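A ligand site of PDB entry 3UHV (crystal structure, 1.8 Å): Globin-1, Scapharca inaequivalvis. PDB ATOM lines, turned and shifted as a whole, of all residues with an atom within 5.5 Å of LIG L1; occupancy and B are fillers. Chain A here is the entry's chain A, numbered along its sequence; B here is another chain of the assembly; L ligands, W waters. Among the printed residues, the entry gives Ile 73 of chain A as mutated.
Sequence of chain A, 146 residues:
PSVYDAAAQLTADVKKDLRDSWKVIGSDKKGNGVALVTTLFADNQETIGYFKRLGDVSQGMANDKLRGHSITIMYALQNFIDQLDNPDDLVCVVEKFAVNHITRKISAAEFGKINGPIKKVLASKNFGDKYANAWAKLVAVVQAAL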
ATOM      1  N   LEU A  36     -15.556  -9.723  14.871  1.00  0.00           N
ATOM      2  CA  LEU A  36     -14.383 -10.265  14.219  1.00  0.00           C
ATOM      3  C   LEU A  36     -13.994 -11.625  14.821  1.00  0.00           C
ATOM      4  O   LEU A  36     -13.809 -12.601  14.099  1.00  0.00           O
ATOM      5  CB  LEU A  36     -13.230  -9.269  14.383  1.00  0.00           C
ATOM      6  CG  LEU A  36     -12.127  -9.235  13.327  1.00  0.00           C
ATOM      7  CD1 LEU A  36     -12.744  -8.928  11.972  1.00  0.00           C
ATOM      8  CD2 LEU A  36     -11.099  -8.166  13.695  1.00  0.00           C
ATOM      9  N   LEU A  40     -14.435 -15.604  13.491  1.00  0.00           N
ATOM     10  CA  LEU A  40     -13.269 -16.466  13.342  1.00  0.00           C
ATOM     11  C   LEU A  40     -13.593 -17.851  13.885  1.00  0.00           C
ATOM     12  O   LEU A  40     -13.275 -18.866  13.251  1.00  0.00           O
ATOM     13  CB  LEU A  40     -12.076 -15.891  14.120  1.00  0.00           C
ATOM     14  CG  LEU A  40     -10.840 -16.787  14.179  1.00  0.00           C
ATOM     15  CD1 LEU A  40     -10.232 -16.933  12.786  1.00  0.00           C
ATOM     16  CD2 LEU A  40      -9.818 -16.190  15.128  1.00  0.00           C
ATOM     17  N   THR A  47      -9.634 -23.190  15.336  1.00  0.00           N
ATOM     18  CA  THR A  47      -8.817 -22.219  16.059  1.00  0.00           C
ATOM     19  C   THR A  47      -9.252 -22.043  17.511  1.00  0.00           C
ATOM     20  O   THR A  47      -8.523 -21.478  18.323  1.00  0.00           O
ATOM     21  CB  THR A  47      -8.835 -20.835  15.375  1.00  0.00           C
ATOM     22  OG1 THR A  47     -10.184 -20.339  15.335  1.00  0.00           O
ATOM     23  CG2 THR A  47      -8.281 -20.933  13.963  1.00  0.00           C
ATOM     24  N   TYR A  50      -6.952 -22.848  20.615  1.00  0.00           N
ATOM     25  CA  TYR A  50      -5.922 -21.933  21.112  1.00  0.00           C
ATOM     26  C   TYR A  50      -6.466 -21.000  22.196  1.00  0.00           C
ATOM     27  O   TYR A  50      -5.691 -20.346  22.894  1.00  0.00           O
ATOM     28  CB  TYR A  50      -5.385 -21.060  19.967  1.00  0.00           C
ATOM     29  CG  TYR A  50      -4.624 -21.795  18.906  1.00  0.00           C
ATOM     30  CD1 TYR A  50      -3.373 -22.354  19.171  1.00  0.00           C
ATOM     31  CD2 TYR A  50      -5.129 -21.907  17.609  1.00  0.00           C
ATOM     32  CE1 TYR A  50      -2.647 -23.004  18.175  1.00  0.00           C
ATOM     33  CE2 TYR A  50      -4.415 -22.565  16.617  1.00  0.00           C
ATOM     34  CZ  TYR A  50      -3.172 -23.115  16.903  1.00  0.00           C
ATOM     35  OH  TYR A  50      -2.459 -23.753  15.921  1.00  0.00           O
ATOM     36  N   PHE A  51      -7.789 -20.952  22.329  1.00  0.00           N
ATOM     37  CA  PHE A  51      -8.431 -20.061  23.288  1.00  0.00           C
ATOM     38  C   PHE A  51      -9.127 -20.749  24.458  1.00  0.00           C
ATOM     39  O   PHE A  51     -10.130 -20.244  24.958  1.00  0.00           O
ATOM     40  CB  PHE A  51      -9.442 -19.190  22.549  1.00  0.00           C
ATOM     41  CG  PHE A  51      -8.826 -18.321  21.479  1.00  0.00           C
ATOM     42  CD1 PHE A  51      -8.367 -17.045  21.785  1.00  0.00           C
ATOM     43  CD2 PHE A  51      -8.704 -18.788  20.174  1.00  0.00           C
ATOM     44  CE1 PHE A  51      -7.798 -16.236  20.806  1.00  0.00           C
ATOM     45  CE2 PHE A  51      -8.130 -17.990  19.187  1.00  0.00           C
ATOM     46  CZ  PHE A  51      -7.679 -16.712  19.498  1.00  0.00           C
ATOM     47  N   ARG A  53      -8.522 -20.794  27.512  1.00  0.00           N
ATOM     48  CA  ARG A  53      -8.635 -19.897  28.663  1.00  0.00           C
ATOM     49  C   ARG A  53      -9.896 -19.046  28.650  1.00  0.00           C
ATOM     50  O   ARG A  53     -10.391 -18.639  29.701  1.00  0.00           O
ATOM     51  CB  ARG A  53      -7.406 -18.987  28.748  1.00  0.00           C
ATOM     52  CG  ARG A  53      -7.292 -18.242  30.078  1.00  0.00           C
ATOM     53  CD  ARG A  53      -6.196 -17.182  30.027  1.00  0.00           C
ATOM     54  NE  ARG A  53      -6.619 -16.021  29.260  1.00  0.00           N
ATOM     55  CZ  ARG A  53      -7.456 -15.081  29.700  1.00  0.00           C
ATOM     56  NH1 ARG A  53      -7.972 -15.168  30.922  1.00  0.00           N
ATOM     57  NH2 ARG A  53      -7.760 -14.049  28.924  1.00  0.00           N
ATOM     58  N   LEU A  54     -10.411 -18.752  27.455  1.00  0.00           N
ATOM     59  CA  LEU A  54     -11.609 -17.926  27.312  1.00  0.00           C
ATOM     60  C   LEU A  54     -12.903 -18.586  27.774  1.00  0.00           C
ATOM     61  O   LEU A  54     -13.889 -17.905  28.028  1.00  0.00           O
ATOM     62  CB  LEU A  54     -11.745 -17.468  25.854  1.00  0.00           C
ATOM     63  CG  LEU A  54     -11.059 -16.159  25.467  1.00  0.00           C
ATOM     64  CD1 LEU A  54      -9.639 -16.115  26.008  1.00  0.00           C
ATOM     65  CD2 LEU A  54     -11.073 -16.006  23.948  1.00  0.00           C
ATOM     66  N   HIS A  69     -10.874  -9.834  25.515  1.00  0.00           N
ATOM     67  CA  HIS A  69      -9.925 -10.143  24.441  1.00  0.00           C
ATOM     68  C   HIS A  69     -10.305  -9.399  23.174  1.00  0.00           C
ATOM     69  O   HIS A  69      -9.451  -8.770  22.528  1.00  0.00           O
ATOM     70  CB  HIS A  69      -9.905 -11.651  24.166  1.00  0.00           C
ATOM     71  CG  HIS A  69      -9.112 -12.031  22.951  1.00  0.00           C
ATOM     72  ND1 HIS A  69      -7.735 -11.990  22.954  1.00  0.00           N
ATOM     73  CD2 HIS A  69      -9.549 -12.431  21.739  1.00  0.00           C
ATOM     74  CE1 HIS A  69      -7.378 -12.359  21.739  1.00  0.00           C
ATOM     75  NE2 HIS A  69      -8.434 -12.637  20.968  1.00  0.00           N
ATOM     76  N   THR A  72      -9.519  -5.699  23.250  1.00  0.00           N
ATOM     77  CA  THR A  72      -8.066  -5.560  23.228  1.00  0.00           C
ATOM     78  C   THR A  72      -7.408  -5.776  21.870  1.00  0.00           C
ATOM     79  O   THR A  72      -6.440  -5.092  21.538  1.00  0.00           O
ATOM     80  CB  THR A  72      -7.417  -6.508  24.249  1.00  0.00           C
ATOM     81  OG1 THR A  72      -7.890  -6.196  25.561  1.00  0.00           O
ATOM     82  CG2 THR A  72      -5.891  -6.362  24.222  1.00  0.00           C
ATOM     83  N   ILE A  73      -7.899  -6.732  21.075  1.00  0.00           N
ATOM     84  CA  ILE A  73      -7.263  -6.965  19.776  1.00  0.00           C
ATOM     85  C   ILE A  73      -7.384  -5.741  18.874  1.00  0.00           C
ATOM     86  O   ILE A  73      -6.532  -5.509  18.022  1.00  0.00           O
ATOM     87  CB  ILE A  73      -7.855  -8.188  19.016  1.00  0.00           C
ATOM     88  CG1 ILE A  73      -9.211  -7.837  18.422  1.00  0.00           C
ATOM     89  CG2 ILE A  73      -7.928  -9.382  19.954  1.00  0.00           C
ATOM     90  CD1 ILE A  73      -9.621  -8.732  17.259  1.00  0.00           C
ATOM     91  N   MET A  74      -8.447  -4.972  19.066  1.00  0.00           N
ATOM     92  CA  MET A  74      -8.691  -3.769  18.258  1.00  0.00           C
ATOM     93  C   MET A  74      -7.664  -2.656  18.494  1.00  0.00           C
ATOM     94  O   MET A  74      -7.445  -1.797  17.621  1.00  0.00           O
ATOM     95  CB  MET A  74     -10.088  -3.241  18.558  1.00  0.00           C
ATOM     96  CG  MET A  74     -11.209  -4.190  18.115  1.00  0.00           C
ATOM     97  SD  MET A  74     -11.130  -4.683  16.364  1.00  0.00           S
ATOM     98  CE  MET A  74     -12.086  -3.360  15.579  1.00  0.00           C
ATOM     99  N   ALA A  76      -4.570  -3.291  18.883  1.00  0.00           N
ATOM    100  CA  ALA A  76      -3.343  -3.715  18.204  1.00  0.00           C
ATOM    101  C   ALA A  76      -3.463  -3.192  16.767  1.00  0.00           C
ATOM    102  O   ALA A  76      -2.496  -2.737  16.169  1.00  0.00           O
ATOM    103  CB  ALA A  76      -3.209  -5.237  18.209  1.00  0.00           C
ATOM    104  N   LEU A  77      -4.673  -3.291  16.219  1.00  0.00           N
ATOM    105  CA  LEU A  77      -4.931  -2.825  14.867  1.00  0.00           C
ATOM    106  C   LEU A  77      -4.783  -1.304  14.837  1.00  0.00           C
ATOM    107  O   LEU A  77      -4.259  -0.747  13.879  1.00  0.00           O
ATOM    108  CB  LEU A  77      -6.331  -3.238  14.415  1.00  0.00           C
ATOM    109  CG  LEU A  77      -6.543  -4.742  14.251  1.00  0.00           C
ATOM    110  CD1 LEU A  77      -7.968  -5.033  13.785  1.00  0.00           C
ATOM    111  CD2 LEU A  77      -5.532  -5.280  13.256  1.00  0.00           C
ATOM    112  N   PHE A  80      -1.156  -0.506  14.613  1.00  0.00           N
ATOM    113  CA  PHE A  80      -0.642  -0.679  13.252  1.00  0.00           C
ATOM    114  C   PHE A  80      -1.024   0.491  12.349  1.00  0.00           C
ATOM    115  O   PHE A  80      -0.174   1.036  11.652  1.00  0.00           O
ATOM    116  CB  PHE A  80      -1.177  -1.978  12.625  1.00  0.00           C
ATOM    117  CG  PHE A  80      -0.781  -3.232  13.363  1.00  0.00           C
ATOM    118  CD1 PHE A  80       0.338  -3.253  14.180  1.00  0.00           C
ATOM    119  CD2 PHE A  80      -1.519  -4.398  13.212  1.00  0.00           C
ATOM    120  CE1 PHE A  80       0.729  -4.419  14.836  1.00  0.00           C
ATOM    121  CE2 PHE A  80      -1.144  -5.568  13.864  1.00  0.00           C
ATOM    122  CZ  PHE A  80      -0.022  -5.579  14.683  1.00  0.00           C
ATOM    123  N   PHE A  97       4.564  -7.368  18.417  1.00  0.00           N
ATOM    124  CA  PHE A  97       3.266  -8.035  18.429  1.00  0.00           C
ATOM    125  C   PHE A  97       3.399  -9.538  18.188  1.00  0.00           C
ATOM    126  O   PHE A  97       2.685 -10.331  18.793  1.00  0.00           O
ATOM    127  CB  PHE A  97       2.360  -7.400  17.380  1.00  0.00           C
ATOM    128  CG  PHE A  97       1.104  -8.170  17.085  1.00  0.00           C
ATOM    129  CD1 PHE A  97       1.113  -9.203  16.152  1.00  0.00           C
ATOM    130  CD2 PHE A  97      -0.078  -7.854  17.734  1.00  0.00           C
ATOM    131  CE1 PHE A  97      -0.054  -9.908  15.858  1.00  0.00           C
ATOM    132  CE2 PHE A  97      -1.244  -8.553  17.455  1.00  0.00           C
ATOM    133  CZ  PHE A  97      -1.241  -9.582  16.515  1.00  0.00           C
ATOM    134  N   ASN A 100       4.498 -12.908  21.291  1.00  0.00           N
ATOM    135  CA  ASN A 100       3.581 -13.794  22.005  1.00  0.00           C
ATOM    136  C   ASN A 100       2.865 -14.799  21.086  1.00  0.00           C
ATOM    137  O   ASN A 100       2.534 -15.903  21.526  1.00  0.00           O
ATOM    138  CB  ASN A 100       2.544 -12.985  22.790  1.00  0.00           C
ATOM    139  CG  ASN A 100       3.161 -12.238  23.967  1.00  0.00           C
ATOM    140  OD1 ASN A 100       4.273 -12.546  24.405  1.00  0.00           O
ATOM    141  ND2 ASN A 100       2.437 -11.253  24.499  1.00  0.00           N
ATOM    142  N   HIS A 101       2.626 -14.419  19.834  1.00  0.00           N
ATOM    143  CA  HIS A 101       1.966 -15.324  18.914  1.00  0.00           C
ATOM    144  C   HIS A 101       2.921 -16.429  18.473  1.00  0.00           C
ATOM    145  O   HIS A 101       2.491 -17.555  18.183  1.00  0.00           O
ATOM    146  CB  HIS A 101       1.403 -14.557  17.699  1.00  0.00           C
ATOM    147  CG  HIS A 101       0.225 -13.693  18.036  1.00  0.00           C
ATOM    148  ND1 HIS A 101       0.319 -12.448  18.623  1.00  0.00           N
ATOM    149  CD2 HIS A 101      -1.104 -13.942  17.913  1.00  0.00           C
ATOM    150  CE1 HIS A 101      -0.936 -11.999  18.845  1.00  0.00           C
ATOM    151  NE2 HIS A 101      -1.833 -12.864  18.430  1.00  0.00           N
ATOM    152  N   ARG A 104       2.985 -18.984  21.145  1.00  0.00           N
ATOM    153  CA  ARG A 104       1.782 -19.802  21.139  1.00  0.00           C
ATOM    154  C   ARG A 104       1.723 -20.770  19.960  1.00  0.00           C
ATOM    155  O   ARG A 104       0.756 -21.505  19.793  1.00  0.00           O
ATOM    156  CB  ARG A 104       0.538 -18.906  21.137  1.00  0.00           C
ATOM    157  CG  ARG A 104       0.473 -17.971  22.326  1.00  0.00           C
ATOM    158  CD  ARG A 104      -0.894 -17.303  22.458  1.00  0.00           C
ATOM    159  NE  ARG A 104      -0.921 -16.405  23.606  1.00  0.00           N
ATOM    160  CZ  ARG A 104      -0.686 -15.095  23.544  1.00  0.00           C
ATOM    161  NH1 ARG A 104      -0.411 -14.525  22.379  1.00  0.00           N
ATOM    162  NH2 ARG A 104      -0.704 -14.377  24.650  1.00  0.00           N
ATOM    163  N   ILE A 106       1.535 -19.992  16.768  1.00  0.00           N
ATOM    164  CA  ILE A 106       0.610 -19.549  15.727  1.00  0.00           C
ATOM    165  C   ILE A 106       1.418 -19.317  14.455  1.00  0.00           C
ATOM    166  O   ILE A 106       2.277 -18.435  14.417  1.00  0.00           O
ATOM    167  CB  ILE A 106      -0.112 -18.242  16.107  1.00  0.00           C
ATOM    168  CG1 ILE A 106      -0.758 -18.377  17.490  1.00  0.00           C
ATOM    169  CG2 ILE A 106      -1.161 -17.894  15.059  1.00  0.00           C
ATOM    170  CD1 ILE A 106      -1.737 -19.534  17.624  1.00  0.00           C
ATOM    171  N   GLU A 110      -1.947 -19.985   9.975  1.00  0.00           N
ATOM    172  CA  GLU A 110      -2.986 -19.971  11.002  1.00  0.00           C
ATOM    173  C   GLU A 110      -3.511 -18.544  11.174  1.00  0.00           C
ATOM    174  O   GLU A 110      -4.722 -18.303  11.203  1.00  0.00           O
ATOM    175  CB  GLU A 110      -2.411 -20.463  12.332  1.00  0.00           C
ATOM    176  CG  GLU A 110      -3.440 -20.959  13.320  1.00  0.00           C
ATOM    177  CD  GLU A 110      -3.915 -22.370  13.010  1.00  0.00           C
ATOM    178  OE1 GLU A 110      -3.071 -23.294  13.022  1.00  0.00           O
ATOM    179  OE2 GLU A 110      -5.124 -22.551  12.742  1.00  0.00           O
ATOM    180  N   PHE A 111      -2.588 -17.600  11.278  1.00  0.00           N
ATOM    181  CA  PHE A 111      -2.918 -16.184  11.462  1.00  0.00           C
ATOM    182  C   PHE A 111      -3.721 -15.651  10.272  1.00  0.00           C
ATOM    183  O   PHE A 111      -4.634 -14.844  10.438  1.00  0.00           O
ATOM    184  CB  PHE A 111      -1.643 -15.363  11.616  1.00  0.00           C
ATOM    185  CG  PHE A 111      -1.876 -13.987  12.167  1.00  0.00           C
ATOM    186  CD1 PHE A 111      -1.973 -13.788  13.543  1.00  0.00           C
ATOM    187  CD2 PHE A 111      -2.038 -12.901  11.313  1.00  0.00           C
ATOM    188  CE1 PHE A 111      -2.227 -12.515  14.057  1.00  0.00           C
ATOM    189  CE2 PHE A 111      -2.301 -11.633  11.817  1.00  0.00           C
ATOM    190  CZ  PHE A 111      -2.390 -11.436  13.188  1.00  0.00           C
ATOM    191  N   ILE A 114      -7.640 -14.932   9.692  1.00  0.00           N
ATOM    192  CA  ILE A 114      -8.376 -13.752  10.121  1.00  0.00           C
ATOM    193  C   ILE A 114      -8.874 -12.929   8.930  1.00  0.00           C
ATOM    194  O   ILE A 114      -9.768 -12.103   9.081  1.00  0.00           O
ATOM    195  CB  ILE A 114      -7.497 -12.847  11.016  1.00  0.00           C
ATOM    196  CG1 ILE A 114      -8.380 -11.875  11.796  1.00  0.00           C
ATOM    197  CG2 ILE A 114      -6.484 -12.075  10.173  1.00  0.00           C
ATOM    198  CD1 ILE A 114      -9.315 -12.564  12.759  1.00  0.00           C
ATOM    199  N   ILE A 118     -12.272 -10.492   8.640  1.00  0.00           N
ATOM    200  CA  ILE A 118     -12.083  -9.090   8.320  1.00  0.00           C
ATOM    201  C   ILE A 118     -12.893  -8.706   7.075  1.00  0.00           C
ATOM    202  O   ILE A 118     -13.568  -7.670   7.061  1.00  0.00           O
ATOM    203  CB  ILE A 118     -10.588  -8.759   8.082  1.00  0.00           C
ATOM    204  CG1 ILE A 118      -9.816  -8.949   9.396  1.00  0.00           C
ATOM    205  CG2 ILE A 118     -10.425  -7.329   7.600  1.00  0.00           C
ATOM    206  CD1 ILE A 118      -8.328  -8.681   9.285  1.00  0.00           C
ATOM    207  N   LYS B  96      -7.763  -9.010  31.424  1.00  0.00           N
ATOM    208  CA  LYS B  96      -7.145  -9.567  30.221  1.00  0.00           C
ATOM    209  C   LYS B  96      -5.681  -9.122  30.186  1.00  0.00           C
ATOM    210  O   LYS B  96      -4.779  -9.914  29.932  1.00  0.00           O
ATOM    211  CB  LYS B  96      -7.903  -9.073  28.983  1.00  0.00           C
ATOM    212  CG  LYS B  96      -7.146  -9.136  27.651  1.00  0.00           C
ATOM    213  CD  LYS B  96      -6.843 -10.550  27.191  1.00  0.00           C
ATOM    214  CE  LYS B  96      -6.103 -10.507  25.857  1.00  0.00           C
ATOM    215  NZ  LYS B  96      -5.846 -11.853  25.280  1.00  0.00           N
ATOM    216  N   VAL B  99      -3.196 -11.022  32.652  1.00  0.00           N
ATOM    217  CA  VAL B  99      -2.815 -12.404  32.338  1.00  0.00           C
ATOM    218  C   VAL B  99      -1.328 -12.609  32.061  1.00  0.00           C
ATOM    219  O   VAL B  99      -0.666 -13.390  32.745  1.00  0.00           O
ATOM    220  CB  VAL B  99      -3.621 -12.943  31.138  1.00  0.00           C
ATOM    221  CG1 VAL B  99      -3.182 -14.361  30.795  1.00  0.00           C
ATOM    222  CG2 VAL B  99      -5.109 -12.925  31.465  1.00  0.00           C
ATOM    223  N   ASN B 100      -0.791 -11.904  31.064  1.00  0.00           N
ATOM    224  CA  ASN B 100       0.618 -12.063  30.719  1.00  0.00           C
ATOM    225  C   ASN B 100       1.564 -11.533  31.786  1.00  0.00           C
ATOM    226  O   ASN B 100       2.667 -12.069  31.964  1.00  0.00           O
ATOM    227  CB  ASN B 100       0.932 -11.367  29.385  1.00  0.00           C
ATOM    228  CG  ASN B 100       0.334 -12.095  28.193  1.00  0.00           C
ATOM    229  OD1 ASN B 100      -0.017 -13.281  28.285  1.00  0.00           O
ATOM    230  ND2 ASN B 100       0.235 -11.405  27.067  1.00  0.00           N
HETATM  231  C1  LIG L   1      -3.766 -12.589  22.317  1.00  0.00           C
HETATM  232  C2  LIG L   1      -4.319  -9.349  18.778  1.00  0.00           C
HETATM  233  C3  LIG L   1      -5.286 -12.926  15.660  1.00  0.00           C
HETATM  234  C4  LIG L   1      -4.361 -16.189  19.080  1.00  0.00           C
HETATM  235  C5  LIG L   1      -3.671 -11.392  21.598  1.00  0.00           C
HETATM  236  C6  LIG L   1      -3.466 -10.067  22.178  1.00  0.00           C
HETATM  237  C7  LIG L   1      -3.645  -9.170  21.180  1.00  0.00           C
HETATM  238  C8  LIG L   1      -3.930  -9.927  19.979  1.00  0.00           C
HETATM  239  C9  LIG L   1      -3.491  -7.655  21.296  1.00  0.00           C
HETATM  240  C10 LIG L   1      -3.081  -9.712  23.606  1.00  0.00           C
HETATM  241  C11 LIG L   1      -1.572  -9.637  23.799  1.00  0.00           C
HETATM  242  C12 LIG L   1      -0.897 -10.994  23.694  1.00  0.00           C
HETATM  243  O1  LIG L   1      -1.070 -11.818  24.619  1.00  0.00           O
HETATM  244  O2  LIG L   1      -0.193 -11.230  22.695  1.00  0.00           O
HETATM  245  C13 LIG L   1      -4.615 -10.045  17.614  1.00  0.00           C
HETATM  246  C14 LIG L   1      -4.972  -9.411  16.356  1.00  0.00           C
HETATM  247  C15 LIG L   1      -5.252 -10.400  15.462  1.00  0.00           C
HETATM  248  C16 LIG L   1      -5.045 -11.660  16.202  1.00  0.00           C
HETATM  249  C17 LIG L   1      -4.925  -7.903  16.088  1.00  0.00           C
HETATM  250  C18 LIG L   1      -5.593 -10.285  14.107  1.00  0.00           C
HETATM  251  C19 LIG L   1      -6.403  -9.244  13.528  1.00  0.00           C
HETATM  252  C20 LIG L   1      -5.019 -14.139  16.295  1.00  0.00           C
HETATM  253  C21 LIG L   1      -5.262 -15.433  15.689  1.00  0.00           C
HETATM  254  C22 LIG L   1      -5.000 -16.372  16.641  1.00  0.00           C
HETATM  255  C23 LIG L   1      -4.555 -15.627  17.824  1.00  0.00           C
HETATM  256  C24 LIG L   1      -5.673 -15.660  14.226  1.00  0.00           C
HETATM  257  C25 LIG L   1      -5.128 -17.768  16.579  1.00  0.00           C
HETATM  258  C26 LIG L   1      -5.524 -18.592  15.467  1.00  0.00           C
HETATM  259  C27 LIG L   1      -4.178 -15.492  20.278  1.00  0.00           C
HETATM  260  C28 LIG L   1      -4.275 -16.101  21.593  1.00  0.00           C
HETATM  261  C29 LIG L   1      -4.184 -15.099  22.498  1.00  0.00           C
HETATM  262  C30 LIG L   1      -3.975 -13.862  21.752  1.00  0.00           C
HETATM  263  C31 LIG L   1      -4.506 -17.585  21.912  1.00  0.00           C
HETATM  264  C32 LIG L   1      -4.363 -15.219  24.001  1.00  0.00           C
HETATM  265  C33 LIG L   1      -5.831 -15.177  24.417  1.00  0.00           C
HETATM  266  C34 LIG L   1      -6.024 -15.182  25.921  1.00  0.00           C
HETATM  267  O3  LIG L   1      -5.693 -16.201  26.559  1.00  0.00           O
HETATM  268  O4  LIG L   1      -6.501 -14.159  26.455  1.00  0.00           O
HETATM  269  N1  LIG L   1      -3.865 -11.284  20.223  1.00  0.00           N
HETATM  270  N2  LIG L   1      -4.596 -11.426  17.492  1.00  0.00           N
HETATM  271  N3  LIG L   1      -4.539 -14.257  17.585  1.00  0.00           N
HETATM  272  N4  LIG L   1      -4.009 -14.111  20.382  1.00  0.00           N
HETATM  273 FE1  LIG L   1      -3.879 -12.799  18.839  1.00  0.00          FE
HETATM  274  C1  LG2 L   2       4.693  -6.482  27.880  1.00  0.00           C
HETATM  275  C2  LG2 L   2       1.859  -2.713  28.919  1.00  0.00           C
HETATM  276  C3  LG2 L   2       4.293  -2.028  33.064  1.00  0.00           C
HETATM  277  C4  LG2 L   2       6.909  -5.970  32.167  1.00  0.00           C
HETATM  278  C5  LG2 L   2       3.637  -5.586  27.861  1.00  0.00           C
HETATM  279  C6  LG2 L   2       2.727  -5.415  26.741  1.00  0.00           C
HETATM  280  C7  LG2 L   2       1.912  -4.381  27.033  1.00  0.00           C
HETATM  281  C8  LG2 L   2       2.330  -3.884  28.330  1.00  0.00           C
HETATM  282  C9  LG2 L   2       0.705  -3.921  26.219  1.00  0.00           C
HETATM  283  C10 LG2 L   2       2.587  -6.304  25.499  1.00  0.00           C
HETATM  284  C11 LG2 L   2       1.573  -7.417  25.728  1.00  0.00           C
HETATM  285  C12 LG2 L   2       2.060  -8.444  26.737  1.00  0.00           C
HETATM  286  O1  LG2 L   2       3.007  -9.190  26.412  1.00  0.00           O
HETATM  287  O2  LG2 L   2       1.501  -8.509  27.843  1.00  0.00           O
HETATM  288  C13 LG2 L   2       2.251  -2.211  30.146  1.00  0.00           C
HETATM  289  C14 LG2 L   2       1.756  -0.953  30.729  1.00  0.00           C
HETATM  290  C15 LG2 L   2       2.475  -0.738  31.863  1.00  0.00           C
HETATM  291  C16 LG2 L   2       3.377  -1.882  32.012  1.00  0.00           C
HETATM  292  C17 LG2 L   2       0.594  -0.103  30.217  1.00  0.00           C
HETATM  293  C18 LG2 L   2       2.415   0.316  32.787  1.00  0.00           C
HETATM  294  C19 LG2 L   2       1.496   1.445  32.859  1.00  0.00           C
HETATM  295  C20 LG2 L   2       5.143  -3.117  33.247  1.00  0.00           C
HETATM  296  C21 LG2 L   2       6.098  -3.258  34.353  1.00  0.00           C
HETATM  297  C22 LG2 L   2       6.852  -4.368  34.101  1.00  0.00           C
HETATM  298  C23 LG2 L   2       6.320  -4.920  32.849  1.00  0.00           C
HETATM  299  C24 LG2 L   2       6.207  -2.299  35.533  1.00  0.00           C
HETATM  300  C25 LG2 L   2       7.908  -4.926  34.836  1.00  0.00           C
HETATM  301  C26 LG2 L   2       8.584  -4.395  35.998  1.00  0.00           C
HETATM  302  C27 LG2 L   2       6.561  -6.435  30.906  1.00  0.00           C
HETATM  303  C28 LG2 L   2       7.356  -7.376  30.133  1.00  0.00           C
HETATM  304  C29 LG2 L   2       6.761  -7.486  28.920  1.00  0.00           C
HETATM  305  C30 LG2 L   2       5.569  -6.639  28.950  1.00  0.00           C
HETATM  306  C31 LG2 L   2       8.656  -8.064  30.534  1.00  0.00           C
HETATM  307  C32 LG2 L   2       7.347  -8.231  27.722  1.00  0.00           C
HETATM  308  C33 LG2 L   2       8.390  -7.359  27.049  1.00  0.00           C
HETATM  309  C34 LG2 L   2       8.993  -8.002  25.814  1.00  0.00           C
HETATM  310  O3  LG2 L   2       9.714  -9.010  25.953  1.00  0.00           O
HETATM  311  O4  LG2 L   2       8.731  -7.495  24.703  1.00  0.00           O
HETATM  312  N1  LG2 L   2       3.334  -4.693  28.873  1.00  0.00           N
HETATM  313  N2  LG2 L   2       3.204  -2.797  30.971  1.00  0.00           N
HETATM  314  N3  LG2 L   2       5.259  -4.170  32.365  1.00  0.00           N
HETATM  315  N4  LG2 L   2       5.477  -5.965  30.171  1.00  0.00           N
HETATM  316 FE1  LG2 L   2       4.073  -4.634  30.778  1.00  0.00          FE
HETATM  317  O   HOH W   1       0.864  -9.371  21.124  1.00  0.00           O
HETATM  318  O   HOH W   2      -3.195 -12.061  26.339  1.00  0.00           O
HETATM  319  O   HOH W   3      -7.530 -13.127  18.270  1.00  0.00           O
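Residues that only touch LIG L1: Tyr 50, Phe 51, Phe 97, Ile 73, Phe 111, His 69, Ile 114, Leu 54, Ala 76, Glu 110, Leu 77, Thr 72, Thr 47 and Ile 106.
Hydrophobic or aromatic side chains within 4 Å of LIG L1: Tyr 50, Phe 51, Leu 54, His 69, Ile 73, Ala 76, Leu 77, Phe 97, His 101, Ile 106, Phe 111 and Ile 114.
Within 4 Å of LIG L1: Thr 47, Tyr 50, Phe 51, Arg 53, Leu 54, His 69, Thr 72, Ile 73, Ala 76, Leu 77, Phe 97, Asn 100 of chain A, His 101, Arg 104, Ile 106, Glu 110, Phe 111, Ile 114, Lys 96 of chain B and Asn 100 of chain B.
Along chain A the residues within 4 Å of LIG L1 span positions 47 to 114.
ND1 of His 101 is in hydrogen-bond range of O of Phe 97 (3.2 Å).
The backbone NH of Ile 106 is in hydrogen-bond range of the backbone carbonyl oxygen of His 101.
The guanidinium group (NH1) of Arg 104 lies close to the backbone carbonyl oxygen (O) of Asn 100 of chain A (3.4 Å).
NZ of Lys 96 of chain B lies within hydrogen-bond range of ND1 of His 69 (3.0 Å).
The side-chain amide nitrogen (ND2) of Asn 100 of chain B sits close to the side-chain amide nitrogen (ND2) of Asn 100 of chain A (3.4 Å).
OH of Tyr 50 is in hydrogen-bond range of OE1 of Glu 110, 3.0 Å away.
Water W1 bridges an oxygen (O2) of LIG L1 and the backbone carbonyl oxygen (O) of Phe 97.
Water W2 lies within hydrogen-bond range of O1 of LIG L1 and NZ of Lys 96 of chain B.
A ring nitrogen (NE2) of His 101 is bound to an iron atom (FE1) of LIG L1 (2.1 Å).
The guanidinium group (NH2) of Arg 104 is in salt-bridge range of an oxygen (O1) of LIG L1 (2.6 Å).
O4 of LIG L1 is in salt-bridge range of NZ of Lys 96 of chain B, at 2.7 Å.
NH2 of Arg 53 lies within salt-bridge range of O4 of LIG L1, 2.8 Å away.
The side-chain amide nitrogen (ND2) of Asn 100 of chain B sits at hydrogen-bond distance from an oxygen (O1) of LIG L1 (2.8 Å).
ND2 of Asn 100 of chain A is in hydrogen-bond range of O2 of LIG L1.
The side-chain amide nitrogen (ND2) of Asn 100 of chain B lies within hydrogen-bond range of an oxygen (O2) of LG2 L2, 3.3 Å away.
The side-chain amide nitrogen of Asn 100 of chain A sits at hydrogen-bond distance from an oxygen (O1) of LG2 L2 (2.9 Å).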
